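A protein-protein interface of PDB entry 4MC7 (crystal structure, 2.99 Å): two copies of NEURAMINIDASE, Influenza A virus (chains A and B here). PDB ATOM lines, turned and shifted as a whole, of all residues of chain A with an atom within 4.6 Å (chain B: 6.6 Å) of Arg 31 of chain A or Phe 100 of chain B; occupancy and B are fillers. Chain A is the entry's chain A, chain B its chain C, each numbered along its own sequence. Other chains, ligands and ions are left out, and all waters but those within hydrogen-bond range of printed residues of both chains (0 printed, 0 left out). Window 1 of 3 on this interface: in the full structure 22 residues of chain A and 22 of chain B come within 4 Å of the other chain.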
ATOM      1  N   THR A  29     -20.819 -17.642  24.856  1.00  0.00           N
ATOM      2  CA  THR A  29     -19.966 -17.535  23.693  1.00  0.00           C
ATOM      3  C   THR A  29     -18.505 -17.502  24.146  1.00  0.00           C
ATOM      4  O   THR A  29     -17.591 -17.683  23.346  1.00  0.00           O
ATOM      5  CB  THR A  29     -20.302 -16.265  22.802  1.00  0.00           C
ATOM      6  OG1 THR A  29     -20.460 -15.092  23.603  1.00  0.00           O
ATOM      7  CG2 THR A  29     -21.565 -16.469  22.022  1.00  0.00           C
ATOM      8  N   TYR A  30     -18.282 -17.238  25.426  1.00  0.00           N
ATOM      9  CA  TYR A  30     -16.935 -17.233  25.949  1.00  0.00           C
ATOM     10  C   TYR A  30     -16.896 -17.418  27.445  1.00  0.00           C
ATOM     11  O   TYR A  30     -17.783 -16.968  28.219  1.00  0.00           O
ATOM     12  CB  TYR A  30     -16.251 -15.927  25.651  1.00  0.00           C
ATOM     13  CG  TYR A  30     -14.912 -15.758  26.363  1.00  0.00           C
ATOM     14  CD1 TYR A  30     -13.760 -16.380  25.883  1.00  0.00           C
ATOM     15  CD2 TYR A  30     -14.803 -14.973  27.520  1.00  0.00           C
ATOM     16  CE1 TYR A  30     -12.560 -16.228  26.519  1.00  0.00           C
ATOM     17  CE2 TYR A  30     -13.580 -14.815  28.168  1.00  0.00           C
ATOM     18  CZ  TYR A  30     -12.473 -15.445  27.660  1.00  0.00           C
ATOM     19  OH  TYR A  30     -11.269 -15.303  28.294  1.00  0.00           O
ATOM     20  N   ARG A  31     -15.813 -18.048  27.856  1.00  0.00           N
ATOM     21  CA  ARG A  31     -15.608 -18.347  29.242  1.00  0.00           C
ATOM     22  C   ARG A  31     -14.105 -18.367  29.532  1.00  0.00           C
ATOM     23  O   ARG A  31     -13.321 -19.102  28.890  1.00  0.00           O
ATOM     24  CB  ARG A  31     -16.276 -19.668  29.546  1.00  0.00           C
ATOM     25  CG  ARG A  31     -15.970 -20.245  30.867  1.00  0.00           C
ATOM     26  CD  ARG A  31     -16.860 -21.457  31.132  1.00  0.00           C
ATOM     27  NE  ARG A  31     -16.631 -22.566  30.205  1.00  0.00           N
ATOM     28  CZ  ARG A  31     -17.061 -23.801  30.408  1.00  0.00           C
ATOM     29  NH1 ARG A  31     -17.744 -24.095  31.510  1.00  0.00           N
ATOM     30  NH2 ARG A  31     -16.803 -24.741  29.514  1.00  0.00           N
ATOM     31  N   GLY A  32     -13.716 -17.527  30.495  1.00  0.00           N
ATOM     32  CA  GLY A  32     -12.328 -17.400  30.910  1.00  0.00           C
ATOM     33  C   GLY A  32     -11.849 -18.680  31.556  1.00  0.00           C
ATOM     34  O   GLY A  32     -12.643 -19.450  32.055  1.00  0.00           O
ATOM     35  N   GLU A  33     -10.544 -18.910  31.545  1.00  0.00           N
ATOM     36  CA  GLU A  33     -10.038 -20.154  32.082  1.00  0.00           C
ATOM     37  C   GLU A  33     -10.086 -20.159  33.602  1.00  0.00           C
ATOM     38  O   GLU A  33     -10.053 -21.218  34.220  1.00  0.00           O
ATOM     39  CB  GLU A  33      -8.640 -20.463  31.549  1.00  0.00           C
ATOM     40  CG  GLU A  33      -8.386 -21.978  31.380  1.00  0.00           C
ATOM     41  CD  GLU A  33      -9.282 -22.663  30.329  1.00  0.00           C
ATOM     42  OE1 GLU A  33      -9.549 -22.066  29.267  1.00  0.00           O
ATOM     43  OE2 GLU A  33      -9.704 -23.816  30.563  1.00  0.00           O
ATOM     44  N   THR A  35     -12.704 -19.381  35.231  1.00  0.00           N
ATOM     45  CA  THR A  35     -14.093 -19.562  35.608  1.00  0.00           C
ATOM     46  C   THR A  35     -14.290 -21.014  36.006  1.00  0.00           C
ATOM     47  O   THR A  35     -15.353 -21.413  36.508  1.00  0.00           O
ATOM     48  CB  THR A  35     -15.032 -19.220  34.446  1.00  0.00           C
ATOM     49  OG1 THR A  35     -14.796 -20.133  33.387  1.00  0.00           O
ATOM     50  CG2 THR A  35     -14.751 -17.837  33.910  1.00  0.00           C
ATOM     51  N   THR A  36     -13.256 -21.810  35.762  1.00  0.00           N
ATOM     52  CA  THR A  36     -13.312 -23.255  35.999  1.00  0.00           C
ATOM     53  C   THR A  36     -12.130 -23.693  36.865  1.00  0.00           C
ATOM     54  O   THR A  36     -12.327 -24.130  37.991  1.00  0.00           O
ATOM     55  CB  THR A  36     -13.365 -24.068  34.663  1.00  0.00           C
ATOM     56  OG1 THR A  36     -12.389 -23.557  33.744  1.00  0.00           O
ATOM     57  CG2 THR A  36     -14.728 -23.954  34.009  1.00  0.00           C
ATOM     58  N   GLY A  90     -11.467 -13.506  24.273  1.00  0.00           N
ATOM     59  CA  GLY A  90     -11.124 -14.881  23.953  1.00  0.00           C
ATOM     60  C   GLY A  90      -9.653 -15.106  24.172  1.00  0.00           C
ATOM     61  O   GLY A  90      -9.181 -16.227  24.159  1.00  0.00           O
ATOM     62  N   LEU A 358     -14.243 -13.679  33.184  1.00  0.00           N
ATOM     63  CA  LEU A 358     -15.430 -13.326  32.459  1.00  0.00           C
ATOM     64  C   LEU A 358     -16.076 -14.550  31.897  1.00  0.00           C
ATOM     65  O   LEU A 358     -15.395 -15.536  31.560  1.00  0.00           O
ATOM     66  CB  LEU A 358     -15.059 -12.424  31.293  1.00  0.00           C
ATOM     67  CG  LEU A 358     -15.075 -10.956  31.594  1.00  0.00           C
ATOM     68  CD1 LEU A 358     -15.200 -10.208  30.291  1.00  0.00           C
ATOM     69  CD2 LEU A 358     -16.297 -10.753  32.432  1.00  0.00           C
ATOM     70  N   ILE A 359     -17.399 -14.473  31.799  1.00  0.00           N
ATOM     71  CA  ILE A 359     -18.160 -15.368  30.952  1.00  0.00           C
ATOM     72  C   ILE A 359     -19.153 -14.490  30.245  1.00  0.00           C
ATOM     73  O   ILE A 359     -19.610 -13.507  30.809  1.00  0.00           O
ATOM     74  CB  ILE A 359     -18.832 -16.511  31.735  1.00  0.00           C
ATOM     75  CG1 ILE A 359     -19.749 -17.286  30.804  1.00  0.00           C
ATOM     76  CG2 ILE A 359     -19.597 -16.001  32.949  1.00  0.00           C
ATOM     77  CD1 ILE A 359     -19.839 -18.734  31.145  1.00  0.00           C
ATOM     78  N   SER B  79     -16.571 -32.777  32.044  1.00  0.00           N
ATOM     79  CA  SER B  79     -17.022 -32.231  30.749  1.00  0.00           C
ATOM     80  C   SER B  79     -17.589 -30.794  30.758  1.00  0.00           C
ATOM     81  O   SER B  79     -17.418 -30.024  29.804  1.00  0.00           O
ATOM     82  CB  SER B  79     -18.046 -33.182  30.111  1.00  0.00           C
ATOM     83  OG  SER B  79     -17.586 -34.524  30.121  1.00  0.00           O
ATOM     84  N   GLU B  80     -18.268 -30.434  31.832  1.00  0.00           N
ATOM     85  CA  GLU B  80     -18.904 -29.126  31.910  1.00  0.00           C
ATOM     86  C   GLU B  80     -17.909 -28.002  32.022  1.00  0.00           C
ATOM     87  O   GLU B  80     -18.260 -26.845  31.807  1.00  0.00           O
ATOM     88  CB  GLU B  80     -19.875 -29.053  33.089  1.00  0.00           C
ATOM     89  CG  GLU B  80     -21.145 -29.889  32.900  1.00  0.00           C
ATOM     90  CD  GLU B  80     -20.891 -31.394  32.966  1.00  0.00           C
ATOM     91  OE1 GLU B  80     -19.877 -31.813  33.573  1.00  0.00           O
ATOM     92  OE2 GLU B  80     -21.712 -32.155  32.408  1.00  0.00           O
ATOM     93  N   GLN B  81     -16.674 -28.344  32.367  1.00  0.00           N
ATOM     94  CA  GLN B  81     -15.631 -27.348  32.563  1.00  0.00           C
ATOM     95  C   GLN B  81     -14.817 -27.164  31.316  1.00  0.00           C
ATOM     96  O   GLN B  81     -13.940 -26.317  31.264  1.00  0.00           O
ATOM     97  CB  GLN B  81     -14.718 -27.735  33.719  1.00  0.00           C
ATOM     98  CG  GLN B  81     -15.422 -27.776  35.083  1.00  0.00           C
ATOM     99  CD  GLN B  81     -14.455 -27.830  36.255  1.00  0.00           C
ATOM    100  OE1 GLN B  81     -13.824 -28.856  36.520  1.00  0.00           O
ATOM    101  NE2 GLN B  81     -14.343 -26.718  36.968  1.00  0.00           N
ATOM    102  N   MET B  82     -15.139 -27.934  30.289  1.00  0.00           N
ATOM    103  CA  MET B  82     -14.285 -28.019  29.127  1.00  0.00           C
ATOM    104  C   MET B  82     -14.653 -27.033  28.029  1.00  0.00           C
ATOM    105  O   MET B  82     -15.828 -26.720  27.811  1.00  0.00           O
ATOM    106  CB  MET B  82     -14.340 -29.425  28.596  1.00  0.00           C
ATOM    107  CG  MET B  82     -13.589 -30.429  29.423  1.00  0.00           C
ATOM    108  SD  MET B  82     -13.830 -32.108  28.792  1.00  0.00           S
ATOM    109  CE  MET B  82     -12.715 -32.999  29.871  1.00  0.00           C
ATOM    110  N   ASN B  83     -13.630 -26.579  27.326  1.00  0.00           N
ATOM    111  CA  ASN B  83     -13.758 -25.582  26.288  1.00  0.00           C
ATOM    112  C   ASN B  83     -13.023 -26.024  25.042  1.00  0.00           C
ATOM    113  O   ASN B  83     -12.077 -26.794  25.131  1.00  0.00           O
ATOM    114  CB  ASN B  83     -13.092 -24.307  26.752  1.00  0.00           C
ATOM    115  CG  ASN B  83     -13.906 -23.558  27.723  1.00  0.00           C
ATOM    116  OD1 ASN B  83     -15.112 -23.480  27.588  1.00  0.00           O
ATOM    117  ND2 ASN B  83     -13.253 -22.968  28.709  1.00  0.00           N
ATOM    118  N   VAL B  84     -13.433 -25.498  23.897  1.00  0.00           N
ATOM    119  CA  VAL B  84     -12.845 -25.899  22.636  1.00  0.00           C
ATOM    120  C   VAL B  84     -11.893 -24.849  22.163  1.00  0.00           C
ATOM    121  O   VAL B  84     -12.306 -23.724  21.884  1.00  0.00           O
ATOM    122  CB  VAL B  84     -13.909 -26.091  21.530  1.00  0.00           C
ATOM    123  CG1 VAL B  84     -13.245 -26.543  20.243  1.00  0.00           C
ATOM    124  CG2 VAL B  84     -14.980 -27.064  21.987  1.00  0.00           C
ATOM    125  N   TYR B  85     -10.627 -25.238  22.044  1.00  0.00           N
ATOM    126  CA  TYR B  85      -9.566 -24.377  21.499  1.00  0.00           C
ATOM    127  C   TYR B  85      -9.045 -24.790  20.142  1.00  0.00           C
ATOM    128  O   TYR B  85      -9.159 -25.949  19.714  1.00  0.00           O
ATOM    129  CB  TYR B  85      -8.405 -24.308  22.463  1.00  0.00           C
ATOM    130  CG  TYR B  85      -8.751 -23.535  23.712  1.00  0.00           C
ATOM    131  CD1 TYR B  85      -8.725 -22.135  23.731  1.00  0.00           C
ATOM    132  CD2 TYR B  85      -9.113 -24.198  24.873  1.00  0.00           C
ATOM    133  CE1 TYR B  85      -9.044 -21.433  24.862  1.00  0.00           C
ATOM    134  CE2 TYR B  85      -9.421 -23.499  26.027  1.00  0.00           C
ATOM    135  CZ  TYR B  85      -9.392 -22.119  26.016  1.00  0.00           C
ATOM    136  OH  TYR B  85      -9.723 -21.429  27.161  1.00  0.00           O
ATOM    137  N   SER B  86      -8.455 -23.817  19.474  1.00  0.00           N
ATOM    138  CA  SER B  86      -7.787 -24.041  18.206  1.00  0.00           C
ATOM    139  C   SER B  86      -6.338 -23.535  18.310  1.00  0.00           C
ATOM    140  O   SER B  86      -6.027 -22.731  19.168  1.00  0.00           O
ATOM    141  CB  SER B  86      -8.552 -23.295  17.120  1.00  0.00           C
ATOM    142  OG  SER B  86      -7.792 -23.225  15.952  1.00  0.00           O
ATOM    143  N   LEU B  98      -3.098 -20.077  21.917  1.00  0.00           N
ATOM    144  CA  LEU B  98      -4.463 -20.616  21.914  1.00  0.00           C
ATOM    145  C   LEU B  98      -5.440 -19.654  21.324  1.00  0.00           C
ATOM    146  O   LEU B  98      -5.306 -18.451  21.469  1.00  0.00           O
ATOM    147  CB  LEU B  98      -4.927 -20.965  23.317  1.00  0.00           C
ATOM    148  CG  LEU B  98      -4.236 -22.134  23.998  1.00  0.00           C
ATOM    149  CD1 LEU B  98      -5.181 -22.668  25.024  1.00  0.00           C
ATOM    150  CD2 LEU B  98      -3.838 -23.248  23.027  1.00  0.00           C
ATOM    151  N   LYS B  99      -6.404 -20.197  20.616  1.00  0.00           N
ATOM    152  CA  LYS B  99      -7.504 -19.415  20.090  1.00  0.00           C
ATOM    153  C   LYS B  99      -8.778 -20.056  20.571  1.00  0.00           C
ATOM    154  O   LYS B  99      -9.119 -21.194  20.161  1.00  0.00           O
ATOM    155  CB  LYS B  99      -7.502 -19.336  18.551  1.00  0.00           C
ATOM    156  CG  LYS B  99      -8.789 -18.720  18.000  1.00  0.00           C
ATOM    157  CD  LYS B  99      -8.590 -18.129  16.625  1.00  0.00           C
ATOM    158  CE  LYS B  99      -9.832 -18.345  15.762  1.00  0.00           C
ATOM    159  NZ  LYS B  99     -10.761 -17.185  15.839  1.00  0.00           N
ATOM    160  N   PHE B 100      -9.476 -19.338  21.447  1.00  0.00           N
ATOM    161  CA  PHE B 100     -10.740 -19.834  21.959  1.00  0.00           C
ATOM    162  C   PHE B 100     -11.707 -20.001  20.806  1.00  0.00           C
ATOM    163  O   PHE B 100     -11.867 -19.081  19.976  1.00  0.00           O
ATOM    164  CB  PHE B 100     -11.326 -18.864  22.962  1.00  0.00           C
ATOM    165  CG  PHE B 100     -12.501 -19.415  23.707  1.00  0.00           C
ATOM    166  CD1 PHE B 100     -13.771 -19.366  23.144  1.00  0.00           C
ATOM    167  CD2 PHE B 100     -12.337 -19.973  24.974  1.00  0.00           C
ATOM    168  CE1 PHE B 100     -14.857 -19.883  23.807  1.00  0.00           C
ATOM    169  CE2 PHE B 100     -13.419 -20.489  25.659  1.00  0.00           C
ATOM    170  CZ  PHE B 100     -14.687 -20.451  25.073  1.00  0.00           C
ATOM    171  N   GLU B 101     -12.360 -21.161  20.749  1.00  0.00           N
ATOM    172  CA  GLU B 101     -13.230 -21.444  19.624  1.00  0.00           C
ATOM    173  C   GLU B 101     -14.669 -21.530  20.028  1.00  0.00           C
ATOM    174  O   GLU B 101     -15.524 -20.992  19.326  1.00  0.00           O
ATOM    175  CB  GLU B 101     -12.799 -22.703  18.885  1.00  0.00           C
ATOM    176  CG  GLU B 101     -11.559 -22.504  17.964  1.00  0.00           C
ATOM    177  CD  GLU B 101     -11.834 -21.686  16.686  1.00  0.00           C
ATOM    178  OE1 GLU B 101     -12.969 -21.168  16.541  1.00  0.00           O
ATOM    179  OE2 GLU B 101     -10.904 -21.562  15.834  1.00  0.00           O
ATOM    180  N   ALA B 102     -14.930 -22.203  21.154  1.00  0.00           N
ATOM    181  CA  ALA B 102     -16.287 -22.330  21.754  1.00  0.00           C
ATOM    182  C   ALA B 102     -16.278 -23.043  23.118  1.00  0.00           C
ATOM    183  O   ALA B 102     -15.227 -23.535  23.542  1.00  0.00           O
ATOM    184  CB  ALA B 102     -17.241 -23.038  20.805  1.00  0.00           C
ATOM    185  N   VAL B 103     -17.433 -23.109  23.794  1.00  0.00           N
ATOM    186  CA  VAL B 103     -17.515 -23.805  25.093  1.00  0.00           C
ATOM    187  C   VAL B 103     -18.138 -25.107  24.789  1.00  0.00           C
ATOM    188  O   VAL B 103     -19.162 -25.135  24.108  1.00  0.00           O
ATOM    189  CB  VAL B 103     -18.446 -23.132  26.127  1.00  0.00           C
ATOM    190  CG1 VAL B 103     -17.848 -21.874  26.656  1.00  0.00           C
ATOM    191  CG2 VAL B 103     -19.776 -22.815  25.485  1.00  0.00           C
ATOM    192  N   GLY B 104     -17.556 -26.184  25.306  1.00  0.00           N
ATOM    193  CA  GLY B 104     -18.038 -27.533  25.014  1.00  0.00           C
ATOM    194  C   GLY B 104     -16.987 -28.592  25.267  1.00  0.00           C
ATOM    195  O   GLY B 104     -15.826 -28.275  25.437  1.00  0.00           O
ATOM    196  N   LEU B 130     -20.910 -22.616  15.427  1.00  0.00           N
ATOM    197  CA  LEU B 130     -20.408 -21.264  15.182  1.00  0.00           C
ATOM    198  C   LEU B 130     -19.545 -21.009  13.935  1.00  0.00           C
ATOM    199  O   LEU B 130     -18.573 -21.715  13.651  1.00  0.00           O
ATOM    200  CB  LEU B 130     -19.885 -20.602  16.453  1.00  0.00           C
ATOM    201  CG  LEU B 130     -18.955 -21.401  17.315  1.00  0.00           C
ATOM    202  CD1 LEU B 130     -17.539 -20.813  17.168  1.00  0.00           C
ATOM    203  CD2 LEU B 130     -19.486 -21.236  18.681  1.00  0.00           C
ATOM    204  N   GLY B 133     -16.491 -17.693  14.531  1.00  0.00           N
ATOM    205  CA  GLY B 133     -16.441 -17.227  15.915  1.00  0.00           C
ATOM    206  C   GLY B 133     -17.760 -16.731  16.499  1.00  0.00           C
ATOM    207  O   GLY B 133     -17.823 -16.446  17.696  1.00  0.00           O
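NH1 of Arg 31 of chain A is in hydrogen-bond range of O of Glu 80 of chain B (2.8 Å). The backbone carbonyl oxygen (O) of Met 82 of chain B sits at hydrogen-bond distance from the guanidinium group (NH2) of Arg 31 of chain A (2.8 Å). OD1 of Asn 83 of chain B is in hydrogen-bond range of NH2 of Arg 31 of chain A, 2.9 Å away. The backbone carbonyl oxygen (O) of Thr 36 of chain A lies within hydrogen-bond range of the side-chain amide nitrogen (NE2) of Gln 81 of chain B, 3.4 Å away. The side-chain hydroxyl of Tyr 85 of chain B lies close to the side-chain carboxylate of Glu 33 of chain A (2.2 Å).
The backbone carbonyl oxygen (O) of Glu 33 of chain A is in hydrogen-bond range of the side-chain hydroxyl (OG1) of Thr 36 of chain A. The backbone carbonyl oxygen (O) of Met 82 of chain B lies within hydrogen-bond range of the backbone NH (N) of Gly 104 of chain B, 3.1 Å away. The backbone carbonyl oxygen (O) of Gly 104 of chain B is in hydrogen-bond range of the backbone NH (N) of Asn 83 of chain B, at 3.4 Å.
Among the printed residues, pairs that only touch across the chains: Thr 29 of chain A with Phe 100 of chain B (3.5 Å), Tyr 30 of chain A with Phe 100 of chain B (3.9 Å), Arg 31 of chain A with Gln 81 of chain B (3.6 Å), Arg 31 of chain A with Phe 100 of chain B (3.5 Å), Arg 31 of chain A with Val 103 of chain B (3.8 Å), Glu 33 of chain A with Asn 83 of chain B (3.9 Å) and Gly 90 of chain A with Phe 100 of chain B (3.6 Å).
Printed residues of chain A within 4 Å of Phe 100 of chain B: Thr 29 (3.5 Å), Tyr 30 (3.9 Å), Arg 31 (3.5 Å) and Gly 90 (3.6 Å). Printed residues of chain B within 4 Å of Thr 36 of chain A: Gln 81. Printed residues of chain A within 4 Å of Glu 80 of chain B: Arg 31. The nearest residue of chain B that does not touch Arg 31 of chain A is Gly 104 of chain B (4.5 Å). The nearest printed residue of chain A that does not touch Phe 100 of chain B is Glu 33 of chain A (5.5 Å).
Printed residues of chain A that touch a printed residue of chain B: Thr 29, Tyr 30, Arg 31, Glu 33, Thr 36 and Gly 90. Hydrophobic or aromatic side chains of chain A within 4 Å of the printed part of chain B: Tyr 30. Of the 17 printed residues of chain B, 7 touch a printed residue of chain A. Hydrophobic or aromatic side chains of chain B that line the printed part of chain A: Tyr 85, Phe 100 and Val 103. Along chain B the printed residues that touch a printed residue of chain A span positions 80 to 103. Among the printed residues, 12 pairs touch across the chains. Among the printed residues, no Asp or Glu carboxylate lies within 4 Å of a Lys or Arg side-chain nitrogen of the other chain.
No position is printed for both chains.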
